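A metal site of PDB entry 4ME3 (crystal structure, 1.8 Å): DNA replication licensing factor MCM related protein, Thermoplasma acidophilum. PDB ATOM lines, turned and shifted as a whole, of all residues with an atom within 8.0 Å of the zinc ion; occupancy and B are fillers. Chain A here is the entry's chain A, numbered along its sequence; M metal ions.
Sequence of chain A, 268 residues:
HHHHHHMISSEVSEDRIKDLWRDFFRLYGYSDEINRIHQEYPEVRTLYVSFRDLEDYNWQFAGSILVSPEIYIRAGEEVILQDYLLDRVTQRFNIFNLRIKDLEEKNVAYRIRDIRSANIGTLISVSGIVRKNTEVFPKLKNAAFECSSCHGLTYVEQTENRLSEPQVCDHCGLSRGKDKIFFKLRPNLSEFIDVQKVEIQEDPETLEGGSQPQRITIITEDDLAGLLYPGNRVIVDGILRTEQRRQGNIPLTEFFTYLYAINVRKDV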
ATOM      1  N   PHE A 145      25.003 -30.835 -22.991  1.00  0.00           N
ATOM      2  CA  PHE A 145      25.615 -29.888 -23.913  1.00  0.00           C
ATOM      3  C   PHE A 145      24.636 -28.766 -24.250  1.00  0.00           C
ATOM      4  O   PHE A 145      23.503 -29.014 -24.657  1.00  0.00           O
ATOM      5  CB  PHE A 145      26.047 -30.594 -25.197  1.00  0.00           C
ATOM      6  CG  PHE A 145      27.254 -31.480 -25.031  1.00  0.00           C
ATOM      7  CD1 PHE A 145      28.531 -30.946 -25.124  1.00  0.00           C
ATOM      8  CD2 PHE A 145      27.106 -32.829 -24.776  1.00  0.00           C
ATOM      9  CE1 PHE A 145      29.640 -31.756 -24.970  1.00  0.00           C
ATOM     10  CE2 PHE A 145      28.217 -33.645 -24.629  1.00  0.00           C
ATOM     11  CZ  PHE A 145      29.479 -33.105 -24.717  1.00  0.00           C
ATOM     12  N   GLU A 146      25.090 -27.520 -24.102  1.00  0.00           N
ATOM     13  CA  GLU A 146      24.238 -26.374 -24.378  1.00  0.00           C
ATOM     14  C   GLU A 146      24.456 -25.845 -25.798  1.00  0.00           C
ATOM     15  O   GLU A 146      25.578 -25.552 -26.194  1.00  0.00           O
ATOM     16  CB  GLU A 146      24.484 -25.266 -23.362  1.00  0.00           C
ATOM     17  CG  GLU A 146      23.690 -23.993 -23.632  1.00  0.00           C
ATOM     18  CD  GLU A 146      23.887 -22.933 -22.570  1.00  0.00           C
ATOM     19  OE1 GLU A 146      24.587 -23.212 -21.574  1.00  0.00           O
ATOM     20  OE2 GLU A 146      23.354 -21.821 -22.737  1.00  0.00           O
ATOM     21  N   CYS A 147      23.361 -25.733 -26.545  1.00  0.00           N
ATOM     22  CA  CYS A 147      23.394 -25.265 -27.924  1.00  0.00           C
ATOM     23  C   CYS A 147      23.710 -23.772 -27.990  1.00  0.00           C
ATOM     24  O   CYS A 147      23.084 -22.971 -27.300  1.00  0.00           O
ATOM     25  CB  CYS A 147      22.050 -25.542 -28.610  1.00  0.00           C
ATOM     26  SG  CYS A 147      21.921 -24.869 -30.289  1.00  0.00           S
ATOM     27  N   SER A 148      24.667 -23.401 -28.829  1.00  0.00           N
ATOM     28  CA  SER A 148      25.061 -22.001 -28.951  1.00  0.00           C
ATOM     29  C   SER A 148      23.941 -21.145 -29.540  1.00  0.00           C
ATOM     30  O   SER A 148      23.937 -19.928 -29.387  1.00  0.00           O
ATOM     31  CB  SER A 148      26.323 -21.859 -29.807  1.00  0.00           C
ATOM     32  OG  SER A 148      26.150 -22.439 -31.088  1.00  0.00           O
ATOM     33  N   SER A 149      22.980 -21.788 -30.197  1.00  0.00           N
ATOM     34  CA  SER A 149      21.896 -21.066 -30.853  1.00  0.00           C
ATOM     35  C   SER A 149      20.666 -20.904 -29.947  1.00  0.00           C
ATOM     36  O   SER A 149      20.299 -19.783 -29.600  1.00  0.00           O
ATOM     37  CB  SER A 149      21.487 -21.769 -32.152  1.00  0.00           C
ATOM     38  OG  SER A 149      20.493 -21.029 -32.838  1.00  0.00           O
ATOM     39  N   CYS A 150      20.042 -22.011 -29.576  1.00  0.00           N
ATOM     40  CA  CYS A 150      18.813 -21.980 -28.783  1.00  0.00           C
ATOM     41  C   CYS A 150      19.082 -22.132 -27.291  1.00  0.00           C
ATOM     42  O   CYS A 150      18.185 -21.979 -26.467  1.00  0.00           O
ATOM     43  CB  CYS A 150      17.841 -23.065 -29.251  1.00  0.00           C
ATOM     44  SG  CYS A 150      18.363 -24.750 -28.864  1.00  0.00           S
ATOM     45  N   HIS A 151      20.322 -22.461 -26.948  1.00  0.00           N
ATOM     46  CA  HIS A 151      20.727 -22.631 -25.555  1.00  0.00           C
ATOM     47  C   HIS A 151      19.980 -23.785 -24.870  1.00  0.00           C
ATOM     48  O   HIS A 151      19.966 -23.888 -23.639  1.00  0.00           O
ATOM     49  CB  HIS A 151      20.537 -21.328 -24.773  1.00  0.00           C
ATOM     50  CG  HIS A 151      21.379 -20.208 -25.273  1.00  0.00           C
ATOM     51  ND1 HIS A 151      22.764 -20.245 -25.225  1.00  0.00           N
ATOM     52  CD2 HIS A 151      21.061 -19.018 -25.847  1.00  0.00           C
ATOM     53  CE1 HIS A 151      23.251 -19.129 -25.740  1.00  0.00           C
ATOM     54  NE2 HIS A 151      22.237 -18.363 -26.121  1.00  0.00           N
ATOM     55  N   GLY A 152      19.392 -24.662 -25.662  1.00  0.00           N
ATOM     56  CA  GLY A 152      18.767 -25.856 -25.138  1.00  0.00           C
ATOM     57  C   GLY A 152      19.815 -26.899 -24.820  1.00  0.00           C
ATOM     58  O   GLY A 152      20.966 -26.771 -25.231  1.00  0.00           O
ATOM     59  N   LEU A 153      19.414 -27.943 -24.092  1.00  0.00           N
ATOM     60  CA  LEU A 153      20.347 -28.975 -23.666  1.00  0.00           C
ATOM     61  C   LEU A 153      20.184 -30.278 -24.427  1.00  0.00           C
ATOM     62  O   LEU A 153      19.090 -30.851 -24.475  1.00  0.00           O
ATOM     63  CB  LEU A 153      20.193 -29.244 -22.168  1.00  0.00           C
ATOM     64  CG  LEU A 153      20.525 -28.077 -21.245  1.00  0.00           C
ATOM     65  CD1 LEU A 153      20.185 -28.439 -19.810  1.00  0.00           C
ATOM     66  CD2 LEU A 153      21.984 -27.685 -21.380  1.00  0.00           C
ATOM     67  N   THR A 154      21.275 -30.737 -25.032  1.00  0.00           N
ATOM     68  CA  THR A 154      21.327 -32.052 -25.650  1.00  0.00           C
ATOM     69  C   THR A 154      22.209 -32.949 -24.792  1.00  0.00           C
ATOM     70  O   THR A 154      23.368 -32.620 -24.516  1.00  0.00           O
ATOM     71  CB  THR A 154      21.952 -31.973 -27.060  1.00  0.00           C
ATOM     72  OG1 THR A 154      21.094 -31.197 -27.905  1.00  0.00           O
ATOM     73  CG2 THR A 154      22.129 -33.365 -27.663  1.00  0.00           C
ATOM     74  N   VAL A 168      24.122 -32.583 -33.786  1.00  0.00           N
ATOM     75  CA  VAL A 168      22.880 -31.858 -34.017  1.00  0.00           C
ATOM     76  C   VAL A 168      22.164 -31.593 -32.687  1.00  0.00           C
ATOM     77  O   VAL A 168      22.177 -32.424 -31.784  1.00  0.00           O
ATOM     78  CB  VAL A 168      21.942 -32.646 -34.956  1.00  0.00           C
ATOM     79  CG1 VAL A 168      21.705 -34.057 -34.423  1.00  0.00           C
ATOM     80  CG2 VAL A 168      20.611 -31.918 -35.121  1.00  0.00           C
ATOM     81  N   CYS A 169      21.531 -30.421 -32.587  1.00  0.00           N
ATOM     82  CA  CYS A 169      20.806 -30.039 -31.383  1.00  0.00           C
ATOM     83  C   CYS A 169      19.463 -30.763 -31.295  1.00  0.00           C
ATOM     84  O   CYS A 169      18.705 -30.782 -32.270  1.00  0.00           O
ATOM     85  CB  CYS A 169      20.596 -28.514 -31.358  1.00  0.00           C
ATOM     86  SG  CYS A 169      19.639 -27.900 -29.945  1.00  0.00           S
ATOM     87  N   ASP A 170      19.174 -31.346 -30.140  1.00  0.00           N
ATOM     88  CA  ASP A 170      17.915 -32.063 -29.942  1.00  0.00           C
ATOM     89  C   ASP A 170      16.722 -31.126 -29.833  1.00  0.00           C
ATOM     90  O   ASP A 170      15.572 -31.573 -29.928  1.00  0.00           O
ATOM     91  CB  ASP A 170      17.977 -32.923 -28.666  1.00  0.00           C
ATOM     92  CG  ASP A 170      18.709 -34.239 -28.881  1.00  0.00           C
ATOM     93  OD1 ASP A 170      18.957 -34.601 -30.044  1.00  0.00           O
ATOM     94  OD2 ASP A 170      19.031 -34.902 -27.871  1.00  0.00           O
ATOM     95  N   HIS A 171      16.979 -29.837 -29.654  1.00  0.00           N
ATOM     96  CA  HIS A 171      15.896 -28.881 -29.416  1.00  0.00           C
ATOM     97  C   HIS A 171      15.563 -28.020 -30.634  1.00  0.00           C
ATOM     98  O   HIS A 171      14.394 -27.709 -30.875  1.00  0.00           O
ATOM     99  CB  HIS A 171      16.222 -27.992 -28.218  1.00  0.00           C
ATOM    100  CG  HIS A 171      16.165 -28.713 -26.904  1.00  0.00           C
ATOM    101  ND1 HIS A 171      14.989 -28.923 -26.216  1.00  0.00           N
ATOM    102  CD2 HIS A 171      17.147 -29.287 -26.163  1.00  0.00           C
ATOM    103  CE1 HIS A 171      15.241 -29.588 -25.109  1.00  0.00           C
ATOM    104  NE2 HIS A 171      16.543 -29.819 -25.051  1.00  0.00           N
ATOM    105  N   CYS A 172      16.581 -27.616 -31.401  1.00  0.00           N
ATOM    106  CA  CYS A 172      16.346 -26.741 -32.553  1.00  0.00           C
ATOM    107  C   CYS A 172      16.715 -27.374 -33.893  1.00  0.00           C
ATOM    108  O   CYS A 172      16.376 -26.848 -34.947  1.00  0.00           O
ATOM    109  CB  CYS A 172      17.097 -25.413 -32.372  1.00  0.00           C
ATOM    110  SG  CYS A 172      18.871 -25.487 -32.664  1.00  0.00           S
ATOM    111  N   GLY A 173      17.422 -28.508 -33.857  1.00  0.00           N
ATOM    112  CA  GLY A 173      17.686 -29.261 -35.068  1.00  0.00           C
ATOM    113  C   GLY A 173      18.853 -28.768 -35.917  1.00  0.00           C
ATOM    114  O   GLY A 173      19.171 -29.381 -36.939  1.00  0.00           O
ATOM    115  N   LEU A 174      19.489 -27.685 -35.504  1.00  0.00           N
ATOM    116  CA  LEU A 174      20.672 -27.192 -36.206  1.00  0.00           C
ATOM    117  C   LEU A 174      21.858 -28.108 -35.900  1.00  0.00           C
ATOM    118  O   LEU A 174      21.833 -28.844 -34.911  1.00  0.00           O
ATOM    119  CB  LEU A 174      20.985 -25.753 -35.793  1.00  0.00           C
ATOM    120  CG  LEU A 174      19.892 -24.730 -36.099  1.00  0.00           C
ATOM    121  CD1 LEU A 174      20.292 -23.355 -35.593  1.00  0.00           C
ATOM    122  CD2 LEU A 174      19.593 -24.670 -37.596  1.00  0.00           C
ATOM    123  N   SER A 175      22.882 -28.063 -36.744  1.00  0.00           N
ATOM    124  CA  SER A 175      24.045 -28.912 -36.562  1.00  0.00           C
ATOM    125  C   SER A 175      25.343 -28.126 -36.682  1.00  0.00           C
ATOM    126  O   SER A 175      25.353 -27.004 -37.209  1.00  0.00           O
ATOM    127  CB  SER A 175      24.049 -30.049 -37.586  1.00  0.00           C
ATOM    128  OG  SER A 175      24.370 -29.565 -38.878  1.00  0.00           O
ATOM    129  N   ILE A 181      27.015 -24.194 -35.614  1.00  0.00           N
ATOM    130  CA  ILE A 181      26.791 -23.974 -34.183  1.00  0.00           C
ATOM    131  C   ILE A 181      27.827 -24.759 -33.388  1.00  0.00           C
ATOM    132  O   ILE A 181      28.471 -25.664 -33.909  1.00  0.00           O
ATOM    133  CB  ILE A 181      25.382 -24.425 -33.743  1.00  0.00           C
ATOM    134  CG1 ILE A 181      25.225 -25.940 -33.901  1.00  0.00           C
ATOM    135  CG2 ILE A 181      24.310 -23.679 -34.536  1.00  0.00           C
ATOM    136  CD1 ILE A 181      23.924 -26.474 -33.323  1.00  0.00           C
ATOM    137  N   PHE A 182      27.984 -24.405 -32.114  1.00  0.00           N
ATOM    138  CA  PHE A 182      28.894 -25.122 -31.234  1.00  0.00           C
ATOM    139  C   PHE A 182      28.208 -25.474 -29.918  1.00  0.00           C
ATOM    140  O   PHE A 182      27.266 -24.807 -29.495  1.00  0.00           O
ATOM    141  CB  PHE A 182      30.163 -24.305 -30.976  1.00  0.00           C
ATOM    142  CG  PHE A 182      29.908 -22.967 -30.338  1.00  0.00           C
ATOM    143  CD1 PHE A 182      29.855 -22.842 -28.963  1.00  0.00           C
ATOM    144  CD2 PHE A 182      29.718 -21.837 -31.121  1.00  0.00           C
ATOM    145  CE1 PHE A 182      29.620 -21.607 -28.379  1.00  0.00           C
ATOM    146  CE2 PHE A 182      29.485 -20.608 -30.546  1.00  0.00           C
ATOM    147  CZ  PHE A 182      29.432 -20.484 -29.170  1.00  0.00           C
ATOM    148  N   PHE A 183      28.701 -26.522 -29.257  1.00  0.00           N
ATOM    149  CA  PHE A 183      28.094 -27.003 -28.018  1.00  0.00           C
ATOM    150  C   PHE A 183      29.011 -26.768 -26.825  1.00  0.00           C
ATOM    151  O   PHE A 183      30.223 -27.007 -26.891  1.00  0.00           O
ATOM    152  CB  PHE A 183      27.768 -28.487 -28.132  1.00  0.00           C
ATOM    153  CG  PHE A 183      26.648 -28.786 -29.100  1.00  0.00           C
ATOM    154  CD1 PHE A 183      25.325 -28.657 -28.705  1.00  0.00           C
ATOM    155  CD2 PHE A 183      26.929 -29.188 -30.396  1.00  0.00           C
ATOM    156  CE1 PHE A 183      24.301 -28.929 -29.591  1.00  0.00           C
ATOM    157  CE2 PHE A 183      25.898 -29.465 -31.279  1.00  0.00           C
ATOM    158  CZ  PHE A 183      24.587 -29.329 -30.875  1.00  0.00           C
HETATM  159 ZN    ZN M   1      19.713 -25.612 -30.504  1.00  0.00          ZN
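SG of Cys 150 is bound to the zinc ion, 2.3 Å away.
SG of Cys 172 binds the zinc ion, at 2.3 Å.
The side-chain sulfur (SG) of Cys 147 is bound to the zinc ion.
The zinc ion is bound by SG of Cys 169 (2.4 Å).
SG of Cys 150 sits close to N of Gly 152 (3.4 Å).
The backbone NH (N) of Leu 174 lies close to the side-chain sulfur (SG) of Cys 172 (3.6 Å).
The side-chain sulfur of Cys 147 sits close to the backbone NH of Ser 149.
O of Cys 147 sits close to ND1 of His 151.
The backbone NH (N) of Cys 147 lies within hydrogen-bond range of the backbone carbonyl oxygen (O) of Gly 152 (2.9 Å).
The side-chain sulfur (SG) of Cys 169 sits close to the backbone NH (N) of His 171 (3.3 Å).
O of Leu 174 sits at hydrogen-bond distance from N of Cys 169 (2.8 Å).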
